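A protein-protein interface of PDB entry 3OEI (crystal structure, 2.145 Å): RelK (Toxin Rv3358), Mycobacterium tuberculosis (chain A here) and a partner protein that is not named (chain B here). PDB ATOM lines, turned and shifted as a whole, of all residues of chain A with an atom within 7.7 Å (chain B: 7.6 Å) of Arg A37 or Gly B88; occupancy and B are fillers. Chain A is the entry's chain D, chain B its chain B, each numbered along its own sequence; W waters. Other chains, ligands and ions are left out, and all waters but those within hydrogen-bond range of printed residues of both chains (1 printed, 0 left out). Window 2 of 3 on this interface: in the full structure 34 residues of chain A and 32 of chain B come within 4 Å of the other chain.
Among the printed residues, merely in contact across the chains: Arg A37 with Gly B88, Arg A37 with Glu B90, Arg A41 with Glu B90, Thr A40 with Arg B84, Arg A37 with Gly B89, Thr A40 with Ala B87, Ile A43 with Leu B83, Thr A40 with Leu B83, Arg A33 with Ala B87, Phe A25 with Leu B83 and Thr A40 with Gly B89.
Water W1 lies within hydrogen-bond range of O of Arg A41 and OE2 of Glu B90.
Of the 10 printed residues of chain B, 8 touch a printed residue of chain A. Hydrophobic or aromatic side chains of chain B that line the printed part of chain A: Leu B83 and Ala B87. Along chain A the printed residues that touch a printed residue of chain B span positions 25 to 43. Among the printed residues, 16 pairs touch across the chains.
The backbone carbonyl oxygen (O) of Ala B87 sits close to the guanidinium group (NH1) of Arg A37, at 3.1 Å. The guanidinium group (NE) of Arg A37 lies within salt-bridge range of the side-chain carboxylate (OE2) of Glu B91, at 2.9 Å. O of Glu B91 is in hydrogen-bond range of NH2 of Arg A38 (2.6 Å). NH1 of Arg A41 is in hydrogen-bond range of O of Glu B91 (3.1 Å). The guanidinium group (NH2) of Arg A33 sits close to the backbone carbonyl oxygen (O) of Met B86 (2.3 Å).
Ala A36 touches none of the printed residues of chain B. Arg A37 touches five residues of chain B. Printed residues of chain A within 4 Å of Gly B88: Arg A37 (3.4 Å). Of the printed residues of chain A, Gly B89 touches Arg A37 and Thr A40. Printed residues of chain A within 4 Å of Glu B90: Arg A37 (3.5 Å) and Arg A41 (3.5 Å). The nearest printed residue of chain A that does not touch Gly B88 is Arg A33 (4.01 Å).
The backbone NH (N) of Gly B89 sits at hydrogen-bond distance from the backbone carbonyl oxygen (O) of Arg B84 (2.8 Å). The side-chain carboxylate (OE1) of Glu B90 is in salt-bridge range of the guanidinium group (NE) of Arg B84 (2.7 Å). The guanidinium group (NH1) of Arg A37 sits close to the backbone carbonyl oxygen (O) of Arg A33 (3.5 Å). The backbone carbonyl oxygen (O) of Ala A36 sits at hydrogen-bond distance from the side-chain hydroxyl (OG1) of Thr A40 (3.0 Å).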
ATOM      1  N   PHE A  25     -20.508  11.997  35.967  1.00  0.00           N
ATOM      2  CA  PHE A  25     -19.543  12.234  34.885  1.00  0.00           C
ATOM      3  C   PHE A  25     -18.393  13.173  35.295  1.00  0.00           C
ATOM      4  O   PHE A  25     -17.211  12.880  35.079  1.00  0.00           O
ATOM      5  CB  PHE A  25     -20.259  12.797  33.665  1.00  0.00           C
ATOM      6  CG  PHE A  25     -19.403  12.847  32.438  1.00  0.00           C
ATOM      7  CD1 PHE A  25     -19.053  11.678  31.776  1.00  0.00           C
ATOM      8  CD2 PHE A  25     -18.951  14.055  31.940  1.00  0.00           C
ATOM      9  CE1 PHE A  25     -18.266  11.721  30.635  1.00  0.00           C
ATOM     10  CE2 PHE A  25     -18.166  14.105  30.796  1.00  0.00           C
ATOM     11  CZ  PHE A  25     -17.822  12.940  30.149  1.00  0.00           C
ATOM     12  N   TRP A  28     -15.975  11.481  37.388  1.00  0.00           N
ATOM     13  CA  TRP A  28     -15.066  10.597  36.676  1.00  0.00           C
ATOM     14  C   TRP A  28     -14.001  11.385  35.904  1.00  0.00           C
ATOM     15  O   TRP A  28     -12.852  10.962  35.829  1.00  0.00           O
ATOM     16  CB  TRP A  28     -15.840   9.665  35.749  1.00  0.00           C
ATOM     17  CG  TRP A  28     -16.594   8.553  36.464  1.00  0.00           C
ATOM     18  CD1 TRP A  28     -17.941   8.325  36.429  1.00  0.00           C
ATOM     19  CD2 TRP A  28     -16.034   7.521  37.291  1.00  0.00           C
ATOM     20  NE1 TRP A  28     -18.254   7.211  37.182  1.00  0.00           N
ATOM     21  CE2 TRP A  28     -17.102   6.700  37.717  1.00  0.00           C
ATOM     22  CE3 TRP A  28     -14.739   7.218  37.717  1.00  0.00           C
ATOM     23  CZ2 TRP A  28     -16.911   5.589  38.542  1.00  0.00           C
ATOM     24  CZ3 TRP A  28     -14.546   6.110  38.540  1.00  0.00           C
ATOM     25  CH2 TRP A  28     -15.633   5.305  38.939  1.00  0.00           C
ATOM     26  N   LEU A  29     -14.381  12.535  35.352  1.00  0.00           N
ATOM     27  CA  LEU A  29     -13.413  13.404  34.694  1.00  0.00           C
ATOM     28  C   LEU A  29     -12.227  13.661  35.617  1.00  0.00           C
ATOM     29  O   LEU A  29     -11.082  13.597  35.183  1.00  0.00           O
ATOM     30  CB  LEU A  29     -14.050  14.720  34.259  1.00  0.00           C
ATOM     31  CG  LEU A  29     -14.797  14.769  32.926  1.00  0.00           C
ATOM     32  CD1 LEU A  29     -15.621  13.544  32.781  1.00  0.00           C
ATOM     33  CD2 LEU A  29     -15.692  15.992  32.862  1.00  0.00           C
ATOM     34  N   ASP A  32     -10.821   9.418  37.122  1.00  0.00           N
ATOM     35  CA  ASP A  32     -10.372   8.432  36.141  1.00  0.00           C
ATOM     36  C   ASP A  32     -10.971   8.739  34.775  1.00  0.00           C
ATOM     37  O   ASP A  32     -12.102   8.360  34.494  1.00  0.00           O
ATOM     38  CB  ASP A  32     -10.754   7.009  36.563  1.00  0.00           C
ATOM     39  CG  ASP A  32     -10.044   5.942  35.721  1.00  0.00           C
ATOM     40  OD1 ASP A  32      -8.789   5.939  35.674  1.00  0.00           O
ATOM     41  OD2 ASP A  32     -10.732   5.116  35.088  1.00  0.00           O
ATOM     42  N   ARG A  33     -10.209   9.436  33.940  1.00  0.00           N
ATOM     43  CA  ARG A  33     -10.688   9.878  32.638  1.00  0.00           C
ATOM     44  C   ARG A  33     -11.007   8.729  31.689  1.00  0.00           C
ATOM     45  O   ARG A  33     -11.821   8.881  30.797  1.00  0.00           O
ATOM     46  CB  ARG A  33      -9.654  10.782  31.976  1.00  0.00           C
ATOM     47  CG  ARG A  33      -9.612  12.212  32.478  1.00  0.00           C
ATOM     48  CD  ARG A  33      -8.546  12.975  31.712  1.00  0.00           C
ATOM     49  NE  ARG A  33      -9.081  13.770  30.612  1.00  0.00           N
ATOM     50  CZ  ARG A  33      -9.881  14.816  30.791  1.00  0.00           C
ATOM     51  NH1 ARG A  33     -10.249  15.167  32.027  1.00  0.00           N
ATOM     52  NH2 ARG A  33     -10.316  15.500  29.740  1.00  0.00           N
ATOM     53  N   LYS A  34     -10.321   7.604  31.864  1.00  0.00           N
ATOM     54  CA  LYS A  34     -10.591   6.390  31.097  1.00  0.00           C
ATOM     55  C   LYS A  34     -12.037   5.931  31.318  1.00  0.00           C
ATOM     56  O   LYS A  34     -12.738   5.582  30.376  1.00  0.00           O
ATOM     57  CB  LYS A  34      -9.627   5.274  31.511  1.00  0.00           C
ATOM     58  CG  LYS A  34      -9.519   4.137  30.519  1.00  0.00           C
ATOM     59  CD  LYS A  34      -8.522   3.085  30.975  1.00  0.00           C
ATOM     60  CE  LYS A  34      -8.285   2.039  29.884  1.00  0.00           C
ATOM     61  NZ  LYS A  34      -7.509   0.861  30.376  1.00  0.00           N
ATOM     62  N   THR A  35     -12.490   5.959  32.564  1.00  0.00           N
ATOM     63  CA  THR A  35     -13.884   5.631  32.886  1.00  0.00           C
ATOM     64  C   THR A  35     -14.865   6.605  32.249  1.00  0.00           C
ATOM     65  O   THR A  35     -15.924   6.207  31.748  1.00  0.00           O
ATOM     66  CB  THR A  35     -14.101   5.609  34.396  1.00  0.00           C
ATOM     67  OG1 THR A  35     -13.268   4.586  34.938  1.00  0.00           O
ATOM     68  CG2 THR A  35     -15.565   5.299  34.730  1.00  0.00           C
ATOM     69  N   ALA A  36     -14.499   7.881  32.243  1.00  0.00           N
ATOM     70  CA  ALA A  36     -15.348   8.869  31.617  1.00  0.00           C
ATOM     71  C   ALA A  36     -15.395   8.627  30.112  1.00  0.00           C
ATOM     72  O   ALA A  36     -16.407   8.898  29.466  1.00  0.00           O
ATOM     73  CB  ALA A  36     -14.866  10.269  31.932  1.00  0.00           C
ATOM     74  N   ARG A  37     -14.302   8.128  29.540  1.00  0.00           N
ATOM     75  CA  ARG A  37     -14.318   7.806  28.112  1.00  0.00           C
ATOM     76  C   ARG A  37     -15.191   6.575  27.833  1.00  0.00           C
ATOM     77  O   ARG A  37     -15.825   6.468  26.777  1.00  0.00           O
ATOM     78  CB  ARG A  37     -12.894   7.681  27.541  1.00  0.00           C
ATOM     79  CG  ARG A  37     -12.153   9.031  27.572  1.00  0.00           C
ATOM     80  CD  ARG A  37     -10.862   9.085  26.736  1.00  0.00           C
ATOM     81  NE  ARG A  37      -9.778   8.289  27.301  1.00  0.00           N
ATOM     82  CZ  ARG A  37      -8.964   8.698  28.269  1.00  0.00           C
ATOM     83  NH1 ARG A  37      -9.124   9.903  28.820  1.00  0.00           N
ATOM     84  NH2 ARG A  37      -8.004   7.889  28.701  1.00  0.00           N
ATOM     85  N   ARG A  38     -15.272   5.663  28.792  1.00  0.00           N
ATOM     86  CA  ARG A  38     -16.152   4.507  28.599  1.00  0.00           C
ATOM     87  C   ARG A  38     -17.599   4.942  28.701  1.00  0.00           C
ATOM     88  O   ARG A  38     -18.454   4.508  27.925  1.00  0.00           O
ATOM     89  CB  ARG A  38     -15.806   3.355  29.546  1.00  0.00           C
ATOM     90  CG  ARG A  38     -16.816   2.179  29.539  1.00  0.00           C
ATOM     91  CD  ARG A  38     -17.110   1.658  28.127  1.00  0.00           C
ATOM     92  NE  ARG A  38     -15.890   1.279  27.423  1.00  0.00           N
ATOM     93  CZ  ARG A  38     -15.253   0.127  27.593  1.00  0.00           C
ATOM     94  NH1 ARG A  38     -15.720  -0.773  28.450  1.00  0.00           N
ATOM     95  NH2 ARG A  38     -14.149  -0.126  26.909  1.00  0.00           N
ATOM     96  N   ILE A  39     -17.870   5.846  29.628  1.00  0.00           N
ATOM     97  CA  ILE A  39     -19.200   6.409  29.734  1.00  0.00           C
ATOM     98  C   ILE A  39     -19.620   7.104  28.452  1.00  0.00           C
ATOM     99  O   ILE A  39     -20.731   6.895  27.956  1.00  0.00           O
ATOM    100  CB  ILE A  39     -19.312   7.357  30.937  1.00  0.00           C
ATOM    101  CG1 ILE A  39     -19.338   6.543  32.236  1.00  0.00           C
ATOM    102  CG2 ILE A  39     -20.578   8.222  30.826  1.00  0.00           C
ATOM    103  CD1 ILE A  39     -18.914   7.344  33.486  1.00  0.00           C
ATOM    104  N   THR A  40     -18.732   7.938  27.915  1.00  0.00           N
ATOM    105  CA  THR A  40     -19.012   8.651  26.668  1.00  0.00           C
ATOM    106  C   THR A  40     -19.283   7.670  25.528  1.00  0.00           C
ATOM    107  O   THR A  40     -20.215   7.851  24.731  1.00  0.00           O
ATOM    108  CB  THR A  40     -17.838   9.589  26.270  1.00  0.00           C
ATOM    109  OG1 THR A  40     -17.620  10.553  27.310  1.00  0.00           O
ATOM    110  CG2 THR A  40     -18.161  10.318  24.981  1.00  0.00           C
ATOM    111  N   ARG A  41     -18.464   6.632  25.446  1.00  0.00           N
ATOM    112  CA  ARG A  41     -18.692   5.601  24.432  1.00  0.00           C
ATOM    113  C   ARG A  41     -20.108   4.980  24.557  1.00  0.00           C
ATOM    114  O   ARG A  41     -20.819   4.830  23.565  1.00  0.00           O
ATOM    115  CB  ARG A  41     -17.606   4.520  24.508  1.00  0.00           C
ATOM    116  CG  ARG A  41     -17.838   3.337  23.575  1.00  0.00           C
ATOM    117  CD  ARG A  41     -16.663   2.364  23.573  1.00  0.00           C
ATOM    118  NE  ARG A  41     -16.931   1.245  22.673  1.00  0.00           N
ATOM    119  CZ  ARG A  41     -16.233   0.117  22.648  1.00  0.00           C
ATOM    120  NH1 ARG A  41     -15.182  -0.043  23.442  1.00  0.00           N
ATOM    121  NH2 ARG A  41     -16.569  -0.839  21.796  1.00  0.00           N
ATOM    122  N   LEU A  42     -20.520   4.651  25.781  1.00  0.00           N
ATOM    123  CA  LEU A  42     -21.831   4.022  26.006  1.00  0.00           C
ATOM    124  C   LEU A  42     -22.982   4.934  25.614  1.00  0.00           C
ATOM    125  O   LEU A  42     -23.954   4.495  24.999  1.00  0.00           O
ATOM    126  CB  LEU A  42     -21.993   3.615  27.477  1.00  0.00           C
ATOM    127  CG  LEU A  42     -21.001   2.548  27.948  1.00  0.00           C
ATOM    128  CD1 LEU A  42     -20.900   2.509  29.475  1.00  0.00           C
ATOM    129  CD2 LEU A  42     -21.371   1.174  27.377  1.00  0.00           C
ATOM    130  N   ILE A  43     -22.871   6.206  25.987  1.00  0.00           N
ATOM    131  CA  ILE A  43     -23.888   7.196  25.657  1.00  0.00           C
ATOM    132  C   ILE A  43     -24.000   7.369  24.143  1.00  0.00           C
ATOM    133  O   ILE A  43     -25.102   7.550  23.613  1.00  0.00           O
ATOM    134  CB  ILE A  43     -23.580   8.543  26.316  1.00  0.00           C
ATOM    135  CG1 ILE A  43     -23.762   8.441  27.826  1.00  0.00           C
ATOM    136  CG2 ILE A  43     -24.463   9.662  25.746  1.00  0.00           C
ATOM    137  CD1 ILE A  43     -23.078   9.539  28.558  1.00  0.00           C
ATOM    138  N   ILE A  72     -20.485  -0.006  33.117  1.00  0.00           N
ATOM    139  CA  ILE A  72     -19.367   0.874  32.851  1.00  0.00           C
ATOM    140  C   ILE A  72     -18.125   0.062  33.151  1.00  0.00           C
ATOM    141  O   ILE A  72     -17.164   0.066  32.394  1.00  0.00           O
ATOM    142  CB  ILE A  72     -19.444   2.130  33.733  1.00  0.00           C
ATOM    143  CG1 ILE A  72     -20.660   2.977  33.320  1.00  0.00           C
ATOM    144  CG2 ILE A  72     -18.136   2.894  33.649  1.00  0.00           C
ATOM    145  CD1 ILE A  72     -21.106   4.019  34.386  1.00  0.00           C
ATOM    146  N   GLU B  82     -19.744  17.359  23.143  1.00  0.00           N
ATOM    147  CA  GLU B  82     -19.335  18.014  24.379  1.00  0.00           C
ATOM    148  C   GLU B  82     -18.660  17.006  25.290  1.00  0.00           C
ATOM    149  O   GLU B  82     -17.614  17.287  25.870  1.00  0.00           O
ATOM    150  CB  GLU B  82     -20.541  18.608  25.115  1.00  0.00           C
ATOM    151  CG  GLU B  82     -21.436  19.482  24.265  1.00  0.00           C
ATOM    152  CD  GLU B  82     -22.559  20.144  25.062  1.00  0.00           C
ATOM    153  OE1 GLU B  82     -23.700  20.179  24.542  1.00  0.00           O
ATOM    154  OE2 GLU B  82     -22.301  20.638  26.194  1.00  0.00           O
ATOM    155  N   LEU B  83     -19.269  15.831  25.428  1.00  0.00           N
ATOM    156  CA  LEU B  83     -18.747  14.841  26.360  1.00  0.00           C
ATOM    157  C   LEU B  83     -17.373  14.372  25.882  1.00  0.00           C
ATOM    158  O   LEU B  83     -16.422  14.281  26.669  1.00  0.00           O
ATOM    159  CB  LEU B  83     -19.719  13.661  26.536  1.00  0.00           C
ATOM    160  CG  LEU B  83     -21.129  14.043  27.008  1.00  0.00           C
ATOM    161  CD1 LEU B  83     -22.033  12.836  27.037  1.00  0.00           C
ATOM    162  CD2 LEU B  83     -21.115  14.727  28.379  1.00  0.00           C
ATOM    163  N   ARG B  84     -17.279  14.092  24.586  1.00  0.00           N
ATOM    164  CA  ARG B  84     -16.029  13.644  23.975  1.00  0.00           C
ATOM    165  C   ARG B  84     -14.892  14.633  24.226  1.00  0.00           C
ATOM    166  O   ARG B  84     -13.791  14.239  24.614  1.00  0.00           O
ATOM    167  CB  ARG B  84     -16.220  13.419  22.470  1.00  0.00           C
ATOM    168  CG  ARG B  84     -17.019  12.186  22.125  1.00  0.00           C
ATOM    169  CD  ARG B  84     -17.644  12.262  20.750  1.00  0.00           C
ATOM    170  NE  ARG B  84     -18.228  10.979  20.362  1.00  0.00           N
ATOM    171  CZ  ARG B  84     -19.356  10.847  19.669  1.00  0.00           C
ATOM    172  NH1 ARG B  84     -20.042  11.924  19.296  1.00  0.00           N
ATOM    173  NH2 ARG B  84     -19.805   9.637  19.353  1.00  0.00           N
ATOM    174  N   GLU B  85     -15.166  15.915  24.002  1.00  0.00           N
ATOM    175  CA  GLU B  85     -14.178  16.971  24.238  1.00  0.00           C
ATOM    176  C   GLU B  85     -13.655  16.924  25.678  1.00  0.00           C
ATOM    177  O   GLU B  85     -12.439  16.963  25.909  1.00  0.00           O
ATOM    178  CB  GLU B  85     -14.790  18.350  23.930  1.00  0.00           C
ATOM    179  CG  GLU B  85     -13.785  19.513  23.849  1.00  0.00           C
ATOM    180  CD  GLU B  85     -13.361  20.059  25.212  1.00  0.00           C
ATOM    181  OE1 GLU B  85     -12.312  20.748  25.278  1.00  0.00           O
ATOM    182  OE2 GLU B  85     -14.077  19.819  26.216  1.00  0.00           O
ATOM    183  N   MET B  86     -14.573  16.820  26.642  1.00  0.00           N
ATOM    184  CA  MET B  86     -14.198  16.837  28.057  1.00  0.00           C
ATOM    185  C   MET B  86     -13.478  15.572  28.470  1.00  0.00           C
ATOM    186  O   MET B  86     -12.611  15.605  29.336  1.00  0.00           O
ATOM    187  CB  MET B  86     -15.419  16.992  28.967  1.00  0.00           C
ATOM    188  CG  MET B  86     -16.331  18.172  28.664  1.00  0.00           C
ATOM    189  SD  MET B  86     -17.654  18.249  29.892  1.00  0.00           S
ATOM    190  CE  MET B  86     -19.015  18.805  28.883  1.00  0.00           C
ATOM    191  N   ALA B  87     -13.864  14.444  27.884  1.00  0.00           N
ATOM    192  CA  ALA B  87     -13.297  13.176  28.317  1.00  0.00           C
ATOM    193  C   ALA B  87     -12.015  12.832  27.544  1.00  0.00           C
ATOM    194  O   ALA B  87     -11.278  11.903  27.916  1.00  0.00           O
ATOM    195  CB  ALA B  87     -14.329  12.069  28.186  1.00  0.00           C
ATOM    196  N   GLY B  88     -11.730  13.609  26.498  1.00  0.00           N
ATOM    197  CA  GLY B  88     -10.579  13.326  25.654  1.00  0.00           C
ATOM    198  C   GLY B  88     -10.843  12.156  24.718  1.00  0.00           C
ATOM    199  O   GLY B  88      -9.957  11.366  24.422  1.00  0.00           O
ATOM    200  N   GLY B  89     -12.083  12.050  24.259  1.00  0.00           N
ATOM    201  CA  GLY B  89     -12.478  10.998  23.348  1.00  0.00           C
ATOM    202  C   GLY B  89     -13.486  10.028  23.943  1.00  0.00           C
ATOM    203  O   GLY B  89     -14.269  10.369  24.844  1.00  0.00           O
ATOM    204  N   GLU B  90     -13.465   8.802  23.427  1.00  0.00           N
ATOM    205  CA  GLU B  90     -14.312   7.748  23.926  1.00  0.00           C
ATOM    206  C   GLU B  90     -13.587   6.431  23.716  1.00  0.00           C
ATOM    207  O   GLU B  90     -12.799   6.290  22.785  1.00  0.00           O
ATOM    208  CB  GLU B  90     -15.656   7.748  23.205  1.00  0.00           C
ATOM    209  CG  GLU B  90     -15.584   7.376  21.722  1.00  0.00           C
ATOM    210  CD  GLU B  90     -16.955   7.415  21.046  1.00  0.00           C
ATOM    211  OE1 GLU B  90     -17.287   8.435  20.398  1.00  0.00           O
ATOM    212  OE2 GLU B  90     -17.699   6.417  21.155  1.00  0.00           O
ATOM    213  N   GLU B  91     -13.837   5.483  24.608  1.00  0.00           N
ATOM    214  CA  GLU B  91     -13.232   4.160  24.521  1.00  0.00           C
ATOM    215  C   GLU B  91     -13.773   3.217  25.590  1.00  0.00           C
ATOM    216  O   GLU B  91     -13.797   2.011  25.385  1.00  0.00           O
ATOM    217  CB  GLU B  91     -11.696   4.233  24.558  1.00  0.00           C
ATOM    218  CG  GLU B  91     -11.059   4.805  25.820  1.00  0.00           C
ATOM    219  CD  GLU B  91      -9.515   4.842  25.743  1.00  0.00           C
ATOM    220  OE1 GLU B  91      -8.917   4.012  25.001  1.00  0.00           O
ATOM    221  OE2 GLU B  91      -8.903   5.698  26.429  1.00  0.00           O
HETATM  222  O   HOH W   1     -19.945   4.657  20.953  1.00  0.00           O
